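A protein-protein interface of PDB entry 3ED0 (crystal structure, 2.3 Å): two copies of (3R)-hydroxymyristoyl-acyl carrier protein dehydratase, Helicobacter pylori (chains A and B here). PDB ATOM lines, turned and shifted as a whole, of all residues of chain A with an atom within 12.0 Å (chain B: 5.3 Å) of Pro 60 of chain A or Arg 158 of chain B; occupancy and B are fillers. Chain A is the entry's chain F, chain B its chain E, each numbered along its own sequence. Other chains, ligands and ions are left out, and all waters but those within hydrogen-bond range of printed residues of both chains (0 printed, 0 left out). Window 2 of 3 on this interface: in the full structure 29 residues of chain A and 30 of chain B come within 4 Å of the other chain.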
ATOM      1  N   PHE A  50      -0.966  32.729  11.327  1.00  0.00           N
ATOM      2  CA  PHE A  50      -0.243  32.303  10.144  1.00  0.00           C
ATOM      3  C   PHE A  50       1.194  31.903  10.508  1.00  0.00           C
ATOM      4  O   PHE A  50       1.803  31.074   9.837  1.00  0.00           O
ATOM      5  CB  PHE A  50      -0.211  33.430   9.105  1.00  0.00           C
ATOM      6  CG  PHE A  50       0.474  33.051   7.823  1.00  0.00           C
ATOM      7  CD1 PHE A  50      -0.156  32.216   6.903  1.00  0.00           C
ATOM      8  CD2 PHE A  50       1.763  33.489   7.551  1.00  0.00           C
ATOM      9  CE1 PHE A  50       0.491  31.823   5.728  1.00  0.00           C
ATOM     10  CE2 PHE A  50       2.414  33.099   6.384  1.00  0.00           C
ATOM     11  CZ  PHE A  50       1.776  32.264   5.469  1.00  0.00           C
ATOM     12  N   GLU A  52       2.698  29.827  12.079  1.00  0.00           N
ATOM     13  CA  GLU A  52       2.850  28.456  12.567  1.00  0.00           C
ATOM     14  C   GLU A  52       3.401  27.627  11.408  1.00  0.00           C
ATOM     15  O   GLU A  52       2.905  27.705  10.288  1.00  0.00           O
ATOM     16  CB  GLU A  52       1.502  27.901  13.057  1.00  0.00           C
ATOM     17  CG  GLU A  52       0.903  28.683  14.227  1.00  0.00           C
ATOM     18  CD  GLU A  52      -0.385  28.072  14.776  1.00  0.00           C
ATOM     19  OE1 GLU A  52      -0.330  26.937  15.299  1.00  0.00           O
ATOM     20  OE2 GLU A  52      -1.451  28.729  14.686  1.00  0.00           O
ATOM     21  N   ASP A  53       4.446  26.854  11.686  1.00  0.00           N
ATOM     22  CA  ASP A  53       5.114  26.028  10.680  1.00  0.00           C
ATOM     23  C   ASP A  53       4.179  25.111   9.881  1.00  0.00           C
ATOM     24  O   ASP A  53       4.367  24.923   8.677  1.00  0.00           O
ATOM     25  CB  ASP A  53       6.216  25.210  11.355  1.00  0.00           C
ATOM     26  CG  ASP A  53       7.271  24.712  10.377  1.00  0.00           C
ATOM     27  OD1 ASP A  53       7.249  25.091   9.186  1.00  0.00           O
ATOM     28  OD2 ASP A  53       8.143  23.940  10.808  1.00  0.00           O
ATOM     29  N   VAL A  54       3.167  24.556  10.547  1.00  0.00           N
ATOM     30  CA  VAL A  54       2.210  23.664   9.887  1.00  0.00           C
ATOM     31  C   VAL A  54       1.644  24.243   8.593  1.00  0.00           C
ATOM     32  O   VAL A  54       1.434  23.511   7.632  1.00  0.00           O
ATOM     33  CB  VAL A  54       0.994  23.326  10.805  1.00  0.00           C
ATOM     34  CG1 VAL A  54       0.068  22.335  10.118  1.00  0.00           C
ATOM     35  CG2 VAL A  54       1.470  22.736  12.087  1.00  0.00           C
ATOM     36  N   PHE A  55       1.396  25.550   8.571  1.00  0.00           N
ATOM     37  CA  PHE A  55       0.820  26.186   7.394  1.00  0.00           C
ATOM     38  C   PHE A  55       1.703  26.209   6.157  1.00  0.00           C
ATOM     39  O   PHE A  55       1.221  26.501   5.068  1.00  0.00           O
ATOM     40  CB  PHE A  55       0.337  27.596   7.737  1.00  0.00           C
ATOM     41  CG  PHE A  55      -0.855  27.607   8.648  1.00  0.00           C
ATOM     42  CD1 PHE A  55      -0.761  28.113   9.944  1.00  0.00           C
ATOM     43  CD2 PHE A  55      -2.068  27.050   8.228  1.00  0.00           C
ATOM     44  CE1 PHE A  55      -1.846  28.062  10.808  1.00  0.00           C
ATOM     45  CE2 PHE A  55      -3.166  26.994   9.088  1.00  0.00           C
ATOM     46  CZ  PHE A  55      -3.054  27.500  10.381  1.00  0.00           C
ATOM     47  N   ASN A  56       2.989  25.909   6.315  1.00  0.00           N
ATOM     48  CA  ASN A  56       3.876  25.860   5.159  1.00  0.00           C
ATOM     49  C   ASN A  56       3.426  24.703   4.258  1.00  0.00           C
ATOM     50  O   ASN A  56       3.573  24.756   3.032  1.00  0.00           O
ATOM     51  CB  ASN A  56       5.336  25.640   5.586  1.00  0.00           C
ATOM     52  CG  ASN A  56       6.008  26.920   6.068  1.00  0.00           C
ATOM     53  OD1 ASN A  56       5.943  27.951   5.401  1.00  0.00           O
ATOM     54  ND2 ASN A  56       6.667  26.852   7.218  1.00  0.00           N
ATOM     55  N   GLY A  57       2.850  23.667   4.867  1.00  0.00           N
ATOM     56  CA  GLY A  57       2.415  22.531   4.083  1.00  0.00           C
ATOM     57  C   GLY A  57       0.930  22.223   4.052  1.00  0.00           C
ATOM     58  O   GLY A  57       0.528  21.276   3.393  1.00  0.00           O
ATOM     59  N   HIS A  58       0.103  23.016   4.725  1.00  0.00           N
ATOM     60  CA  HIS A  58      -1.325  22.712   4.747  1.00  0.00           C
ATOM     61  C   HIS A  58      -2.262  23.921   4.646  1.00  0.00           C
ATOM     62  O   HIS A  58      -2.869  24.309   5.642  1.00  0.00           O
ATOM     63  CB  HIS A  58      -1.629  21.922   6.027  1.00  0.00           C
ATOM     64  CG  HIS A  58      -2.946  21.211   6.010  1.00  0.00           C
ATOM     65  ND1 HIS A  58      -4.143  21.852   6.231  1.00  0.00           N
ATOM     66  CD2 HIS A  58      -3.250  19.908   5.804  1.00  0.00           C
ATOM     67  CE1 HIS A  58      -5.129  20.975   6.167  1.00  0.00           C
ATOM     68  NE2 HIS A  58      -4.613  19.787   5.909  1.00  0.00           N
ATOM     69  N   PHE A  59      -2.382  24.528   3.467  1.00  0.00           N
ATOM     70  CA  PHE A  59      -1.668  24.133   2.258  1.00  0.00           C
ATOM     71  C   PHE A  59      -0.989  25.376   1.702  1.00  0.00           C
ATOM     72  O   PHE A  59      -1.323  26.496   2.081  1.00  0.00           O
ATOM     73  CB  PHE A  59      -2.633  23.596   1.187  1.00  0.00           C
ATOM     74  CG  PHE A  59      -3.444  22.413   1.625  1.00  0.00           C
ATOM     75  CD1 PHE A  59      -4.665  22.588   2.271  1.00  0.00           C
ATOM     76  CD2 PHE A  59      -2.979  21.115   1.406  1.00  0.00           C
ATOM     77  CE1 PHE A  59      -5.413  21.493   2.693  1.00  0.00           C
ATOM     78  CE2 PHE A  59      -3.723  20.013   1.826  1.00  0.00           C
ATOM     79  CZ  PHE A  59      -4.946  20.205   2.473  1.00  0.00           C
ATOM     80  N   PRO A  60      -0.021  25.200   0.794  1.00  0.00           N
ATOM     81  CA  PRO A  60       0.645  26.378   0.235  1.00  0.00           C
ATOM     82  C   PRO A  60      -0.387  27.334  -0.373  1.00  0.00           C
ATOM     83  O   PRO A  60      -1.300  26.896  -1.084  1.00  0.00           O
ATOM     84  CB  PRO A  60       1.566  25.772  -0.818  1.00  0.00           C
ATOM     85  CG  PRO A  60       1.929  24.451  -0.212  1.00  0.00           C
ATOM     86  CD  PRO A  60       0.607  23.956   0.310  1.00  0.00           C
ATOM     87  N   ASN A  61      -0.254  28.630  -0.092  1.00  0.00           N
ATOM     88  CA  ASN A  61      -1.188  29.619  -0.639  1.00  0.00           C
ATOM     89  C   ASN A  61      -2.628  29.440  -0.174  1.00  0.00           C
ATOM     90  O   ASN A  61      -3.536  30.071  -0.717  1.00  0.00           O
ATOM     91  CB  ASN A  61      -1.181  29.558  -2.166  1.00  0.00           C
ATOM     92  CG  ASN A  61      -0.097  30.413  -2.780  1.00  0.00           C
ATOM     93  OD1 ASN A  61       1.056  30.395  -2.337  1.00  0.00           O
ATOM     94  ND2 ASN A  61      -0.461  31.168  -3.823  1.00  0.00           N
ATOM     95  N   LYS A  62      -2.844  28.581   0.815  1.00  0.00           N
ATOM     96  CA  LYS A  62      -4.193  28.322   1.317  1.00  0.00           C
ATOM     97  C   LYS A  62      -4.065  27.719   2.719  1.00  0.00           C
ATOM     98  O   LYS A  62      -4.124  26.506   2.892  1.00  0.00           O
ATOM     99  CB  LYS A  62      -4.902  27.345   0.369  1.00  0.00           C
ATOM    100  CG  LYS A  62      -6.324  26.964   0.757  1.00  0.00           C
ATOM    101  CD  LYS A  62      -7.325  27.996   0.302  1.00  0.00           C
ATOM    102  CE  LYS A  62      -8.742  27.601   0.693  1.00  0.00           C
ATOM    103  NZ  LYS A  62      -9.740  28.633   0.251  1.00  0.00           N
ATOM    104  N   PRO A  63      -3.884  28.575   3.739  1.00  0.00           N
ATOM    105  CA  PRO A  63      -3.736  28.145   5.135  1.00  0.00           C
ATOM    106  C   PRO A  63      -5.007  27.626   5.787  1.00  0.00           C
ATOM    107  O   PRO A  63      -5.977  28.363   5.970  1.00  0.00           O
ATOM    108  CB  PRO A  63      -3.197  29.394   5.823  1.00  0.00           C
ATOM    109  CG  PRO A  63      -3.893  30.495   5.065  1.00  0.00           C
ATOM    110  CD  PRO A  63      -3.755  30.040   3.627  1.00  0.00           C
ATOM    111  N   ILE A  64      -4.981  26.345   6.133  1.00  0.00           N
ATOM    112  CA  ILE A  64      -6.103  25.672   6.775  1.00  0.00           C
ATOM    113  C   ILE A  64      -5.559  24.800   7.917  1.00  0.00           C
ATOM    114  O   ILE A  64      -4.781  23.873   7.682  1.00  0.00           O
ATOM    115  CB  ILE A  64      -6.860  24.809   5.740  1.00  0.00           C
ATOM    116  CG1 ILE A  64      -7.503  25.727   4.697  1.00  0.00           C
ATOM    117  CG2 ILE A  64      -7.906  23.943   6.419  1.00  0.00           C
ATOM    118  CD1 ILE A  64      -8.206  24.995   3.592  1.00  0.00           C
ATOM    119  N   PHE A  65      -5.944  25.114   9.151  1.00  0.00           N
ATOM    120  CA  PHE A  65      -5.471  24.347  10.301  1.00  0.00           C
ATOM    121  C   PHE A  65      -5.974  22.919  10.108  1.00  0.00           C
ATOM    122  O   PHE A  65      -7.164  22.703   9.894  1.00  0.00           O
ATOM    123  CB  PHE A  65      -6.021  24.940  11.601  1.00  0.00           C
ATOM    124  CG  PHE A  65      -5.312  24.461  12.845  1.00  0.00           C
ATOM    125  CD1 PHE A  65      -3.990  24.830  13.100  1.00  0.00           C
ATOM    126  CD2 PHE A  65      -5.970  23.647  13.769  1.00  0.00           C
ATOM    127  CE1 PHE A  65      -3.332  24.398  14.261  1.00  0.00           C
ATOM    128  CE2 PHE A  65      -5.329  23.207  14.931  1.00  0.00           C
ATOM    129  CZ  PHE A  65      -4.005  23.583  15.180  1.00  0.00           C
ATOM    130  N   PRO A  66      -5.071  21.925  10.180  1.00  0.00           N
ATOM    131  CA  PRO A  66      -5.452  20.517   9.996  1.00  0.00           C
ATOM    132  C   PRO A  66      -6.532  19.969  10.927  1.00  0.00           C
ATOM    133  O   PRO A  66      -6.449  20.088  12.149  1.00  0.00           O
ATOM    134  CB  PRO A  66      -4.119  19.774  10.153  1.00  0.00           C
ATOM    135  CG  PRO A  66      -3.111  20.786   9.690  1.00  0.00           C
ATOM    136  CD  PRO A  66      -3.613  22.042  10.364  1.00  0.00           C
ATOM    137  N   PRO A 112     -13.882  25.146   8.069  1.00  0.00           N
ATOM    138  CA  PRO A 112     -12.419  25.177   8.130  1.00  0.00           C
ATOM    139  C   PRO A 112     -11.933  26.255   9.097  1.00  0.00           C
ATOM    140  O   PRO A 112     -12.512  27.336   9.174  1.00  0.00           O
ATOM    141  CB  PRO A 112     -12.021  25.475   6.685  1.00  0.00           C
ATOM    142  CG  PRO A 112     -13.163  26.291   6.184  1.00  0.00           C
ATOM    143  CD  PRO A 112     -14.361  25.554   6.737  1.00  0.00           C
ATOM    144  N   THR A 114      -8.870  28.760  10.273  1.00  0.00           N
ATOM    145  CA  THR A 114      -7.790  29.439   9.567  1.00  0.00           C
ATOM    146  C   THR A 114      -7.081  30.464  10.449  1.00  0.00           C
ATOM    147  O   THR A 114      -7.542  30.762  11.548  1.00  0.00           O
ATOM    148  CB  THR A 114      -8.346  30.184   8.328  1.00  0.00           C
ATOM    149  OG1 THR A 114      -9.149  31.286   8.769  1.00  0.00           O
ATOM    150  CG2 THR A 114      -9.202  29.256   7.469  1.00  0.00           C
ATOM    151  N   PRO A 115      -5.951  31.019   9.972  1.00  0.00           N
ATOM    152  CA  PRO A 115      -5.197  32.020  10.740  1.00  0.00           C
ATOM    153  C   PRO A 115      -6.108  33.181  11.142  1.00  0.00           C
ATOM    154  O   PRO A 115      -6.859  33.709  10.315  1.00  0.00           O
ATOM    155  CB  PRO A 115      -4.103  32.449   9.762  1.00  0.00           C
ATOM    156  CG  PRO A 115      -3.839  31.188   9.005  1.00  0.00           C
ATOM    157  CD  PRO A 115      -5.247  30.688   8.722  1.00  0.00           C
ATOM    158  N   PRO B  22      -1.585  17.756  -2.644  1.00  0.00           N
ATOM    159  CA  PRO B  22      -1.245  19.168  -2.458  1.00  0.00           C
ATOM    160  C   PRO B  22      -0.448  19.424  -1.181  1.00  0.00           C
ATOM    161  O   PRO B  22       0.130  20.496  -1.015  1.00  0.00           O
ATOM    162  CB  PRO B  22      -2.612  19.841  -2.433  1.00  0.00           C
ATOM    163  CG  PRO B  22      -3.440  18.827  -1.716  1.00  0.00           C
ATOM    164  CD  PRO B  22      -3.009  17.514  -2.342  1.00  0.00           C
ATOM    165  N   ARG B  24       2.387  19.549   1.690  1.00  0.00           N
ATOM    166  CA  ARG B  24       3.816  19.811   1.652  1.00  0.00           C
ATOM    167  C   ARG B  24       4.401  19.758   3.054  1.00  0.00           C
ATOM    168  O   ARG B  24       3.675  19.532   4.022  1.00  0.00           O
ATOM    169  CB  ARG B  24       4.091  21.168   1.005  1.00  0.00           C
ATOM    170  CG  ARG B  24       3.914  21.157  -0.510  1.00  0.00           C
ATOM    171  CD  ARG B  24       4.868  20.164  -1.169  1.00  0.00           C
ATOM    172  NE  ARG B  24       4.775  20.181  -2.625  1.00  0.00           N
ATOM    173  CZ  ARG B  24       3.870  19.512  -3.338  1.00  0.00           C
ATOM    174  NH1 ARG B  24       3.873  19.604  -4.663  1.00  0.00           N
ATOM    175  NH2 ARG B  24       2.972  18.739  -2.734  1.00  0.00           N
ATOM    176  N   ALA B  94      -4.142  18.110 -10.841  1.00  0.00           N
ATOM    177  CA  ALA B  94      -3.936  18.036  -9.391  1.00  0.00           C
ATOM    178  C   ALA B  94      -3.435  19.343  -8.776  1.00  0.00           C
ATOM    179  O   ALA B  94      -3.757  19.658  -7.636  1.00  0.00           O
ATOM    180  CB  ALA B  94      -2.963  16.895  -9.060  1.00  0.00           C
ATOM    181  N   LYS B  95      -2.653  20.097  -9.538  1.00  0.00           N
ATOM    182  CA  LYS B  95      -2.095  21.371  -9.089  1.00  0.00           C
ATOM    183  C   LYS B  95      -3.033  22.286  -8.314  1.00  0.00           C
ATOM    184  O   LYS B  95      -2.634  22.893  -7.320  1.00  0.00           O
ATOM    185  CB  LYS B  95      -1.583  22.157 -10.293  1.00  0.00           C
ATOM    186  CG  LYS B  95      -0.095  22.061 -10.554  1.00  0.00           C
ATOM    187  CD  LYS B  95       0.208  22.476 -11.989  1.00  0.00           C
ATOM    188  CE  LYS B  95      -0.587  23.710 -12.384  1.00  0.00           C
ATOM    189  NZ  LYS B  95      -0.491  23.986 -13.855  1.00  0.00           N
ATOM    190  N   THR B  96      -4.273  22.402  -8.776  1.00  0.00           N
ATOM    191  CA  THR B  96      -5.232  23.295  -8.138  1.00  0.00           C
ATOM    192  C   THR B  96      -6.283  22.638  -7.255  1.00  0.00           C
ATOM    193  O   THR B  96      -7.331  23.244  -6.992  1.00  0.00           O
ATOM    194  CB  THR B  96      -5.969  24.143  -9.198  1.00  0.00           C
ATOM    195  OG1 THR B  96      -6.655  23.270 -10.108  1.00  0.00           O
ATOM    196  CG2 THR B  96      -4.980  25.015  -9.975  1.00  0.00           C
ATOM    197  N   LYS B  97      -6.018  21.415  -6.796  1.00  0.00           N
ATOM    198  CA  LYS B  97      -6.971  20.715  -5.934  1.00  0.00           C
ATOM    199  C   LYS B  97      -6.528  20.742  -4.467  1.00  0.00           C
ATOM    200  O   LYS B  97      -5.341  20.864  -4.156  1.00  0.00           O
ATOM    201  CB  LYS B  97      -7.137  19.259  -6.369  1.00  0.00           C
ATOM    202  CG  LYS B  97      -7.497  19.053  -7.825  1.00  0.00           C
ATOM    203  CD  LYS B  97      -8.908  19.503  -8.135  1.00  0.00           C
ATOM    204  CE  LYS B  97      -9.233  19.248  -9.596  1.00  0.00           C
ATOM    205  NZ  LYS B  97     -10.533  19.852 -10.003  1.00  0.00           N
ATOM    206  N   ILE B  98      -7.502  20.614  -3.574  1.00  0.00           N
ATOM    207  CA  ILE B  98      -7.272  20.610  -2.134  1.00  0.00           C
ATOM    208  C   ILE B  98      -8.044  19.394  -1.641  1.00  0.00           C
ATOM    209  O   ILE B  98      -8.844  18.826  -2.392  1.00  0.00           O
ATOM    210  CB  ILE B  98      -7.854  21.906  -1.468  1.00  0.00           C
ATOM    211  CG1 ILE B  98      -6.994  23.120  -1.823  1.00  0.00           C
ATOM    212  CG2 ILE B  98      -7.904  21.764   0.054  1.00  0.00           C
ATOM    213  CD1 ILE B  98      -5.555  23.020  -1.348  1.00  0.00           C
ATOM    214  N   ALA B 156     -11.398  19.021  -3.492  1.00  0.00           N
ATOM    215  CA  ALA B 156     -11.991  20.267  -3.959  1.00  0.00           C
ATOM    216  C   ALA B 156     -11.041  21.193  -4.715  1.00  0.00           C
ATOM    217  O   ALA B 156      -9.862  21.321  -4.372  1.00  0.00           O
ATOM    218  CB  ALA B 156     -12.592  21.009  -2.781  1.00  0.00           C
ATOM    219  N   GLU B 157     -11.572  21.841  -5.745  1.00  0.00           N
ATOM    220  CA  GLU B 157     -10.805  22.786  -6.554  1.00  0.00           C
ATOM    221  C   GLU B 157     -10.500  24.027  -5.698  1.00  0.00           C
ATOM    222  O   GLU B 157     -11.377  24.538  -5.002  1.00  0.00           O
ATOM    223  CB  GLU B 157     -11.636  23.187  -7.779  1.00  0.00           C
ATOM    224  CG  GLU B 157     -10.997  24.188  -8.741  1.00  0.00           C
ATOM    225  CD  GLU B 157      -9.856  23.591  -9.553  1.00  0.00           C
ATOM    226  OE1 GLU B 157      -9.854  22.361  -9.768  1.00  0.00           O
ATOM    227  OE2 GLU B 157      -8.972  24.356  -9.991  1.00  0.00           O
ATOM    228  N   ARG B 158      -9.258  24.497  -5.729  1.00  0.00           N
ATOM    229  CA  ARG B 158      -8.891  25.695  -4.972  1.00  0.00           C
ATOM    230  C   ARG B 158      -9.687  26.872  -5.547  1.00  0.00           C
ATOM    231  O   ARG B 158      -9.560  27.191  -6.738  1.00  0.00           O
ATOM    232  CB  ARG B 158      -7.403  26.025  -5.147  1.00  0.00           C
ATOM    233  CG  ARG B 158      -6.375  25.266  -4.300  1.00  0.00           C
ATOM    234  CD  ARG B 158      -4.974  25.792  -4.688  1.00  0.00           C
ATOM    235  NE  ARG B 158      -3.932  25.585  -3.680  1.00  0.00           N
ATOM    236  CZ  ARG B 158      -3.262  24.445  -3.498  1.00  0.00           C
ATOM    237  NH1 ARG B 158      -3.519  23.370  -4.261  1.00  0.00           N
ATOM    238  NH2 ARG B 158      -2.318  24.381  -2.560  1.00  0.00           N
ATOM    239  N   GLU B 159     -10.518  27.519  -4.738  1.00  0.00           N
ATOM    240  CA  GLU B 159     -11.237  28.662  -5.275  1.00  0.00           C
ATOM    241  C   GLU B 159     -11.054  29.887  -4.411  1.00  0.00           C
ATOM    242  O   GLU B 159     -10.075  29.893  -3.622  1.00  0.00           O
ATOM    243  CB  GLU B 159     -12.728  28.355  -5.502  1.00  0.00           C
ATOM    244  CG  GLU B 159     -13.489  27.723  -4.353  1.00  0.00           C
ATOM    245  CD  GLU B 159     -14.921  27.371  -4.752  1.00  0.00           C
ATOM    246  OE1 GLU B 159     -15.681  28.296  -5.122  1.00  0.00           O
ATOM    247  OE2 GLU B 159     -15.290  26.170  -4.707  1.00  0.00           O
ATOM    248  OXT GLU B 159     -11.858  30.836  -4.566  1.00  0.00           O
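The backbone NH (N) of Arg 24 of chain B is in hydrogen-bond range of the backbone carbonyl oxygen (O) of Gly 57 of chain A (3.1 Å).
The guanidinium group (NH2) of Arg 158 of chain B lies within hydrogen-bond range of the backbone carbonyl oxygen (O) of Pro 60 of chain A (3.1 Å).
Among the printed residues, merely in contact across the chains: Phe 59 of chain A with Ile 98 of chain B, Pro 60 of chain A with Pro 22 of chain B, Phe 59 of chain A with Pro 22 of chain B, Phe 59 of chain A with Arg 158 of chain B and Pro 60 of chain A with Arg 24 of chain B.
Of chain B, only Pro 22, Arg 24 and Arg 158 come within 4 Å of Pro 60 of chain A.
Printed residues of chain A within 4 Å of Arg 158 of chain B: Phe 59 and Pro 60.
Printed residues of chain A within 4 Å of Pro 22 of chain B: Phe 59 and Pro 60.
Of chain A, only Gly 57 and Pro 60 come within 4 Å of Arg 24 of chain B.
No residue of chain A comes within 4 Å of Thr 96 of chain B.
No residue of chain A comes within 4 Å of Lys 97 of chain B.
Of chain A, only Phe 59 (3.6 Å) comes within 4 Å of Ile 98 of chain B.
No residue of chain A comes within 4 Å of Ala 156 of chain B.
No residue of chain A comes within 4 Å of Glu 159 of chain B.
Printed residues of chain B within 4 Å of Gly 57 of chain A: Arg 24.
Of the printed residues of chain B, Phe 59 of chain A touches Pro 22 (3.7 Å), Ile 98 (3.6 Å) and Arg 158 (3.8 Å).
Ile 64 of chain A touches none of the printed residues of chain B.
Asn 61 of chain A touches none of the printed residues of chain B.
The nearest residue of chain A that does not touch Arg 158 of chain B is Lys 62 of chain A (4.5 Å).
The nearest printed residue of chain B that does not touch Gly 57 of chain A is Pro 22 of chain B (4.5 Å).
Hydrophobic or aromatic side chains of chain A that line the printed part of chain B: Phe 59 and Pro 60.
Printed residues of chain B that touch a printed residue of chain A: Pro 22, Arg 24, Ile 98 and Arg 158.
Hydrophobic or aromatic side chains of chain B within 4 Å of the printed part of chain A: Pro 22 and Ile 98.
Among the printed residues, no Asp or Glu carboxylate lies within 4 Å of a Lys or Arg side-chain nitrogen of the other chain.
No position is printed for both chains.
Of the 7 pairs that touch across the chains among the printed residues, none has its exchanged pair printed and touching as well.
O of Lys 97 of chain B is in hydrogen-bond range of NH1 of Arg 158 of chain B, at 3.1 Å.
O of Thr 96 of chain B is in hydrogen-bond range of N of Arg 158 of chain B (2.6 Å).
O of Lys 95 of chain B is in hydrogen-bond range of NH1 of Arg 158 of chain B, 3.2 Å away.
The backbone NH (N) of Ile 98 of chain B sits at hydrogen-bond distance from the backbone carbonyl oxygen (O) of Ala 156 of chain B (2.6 Å).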
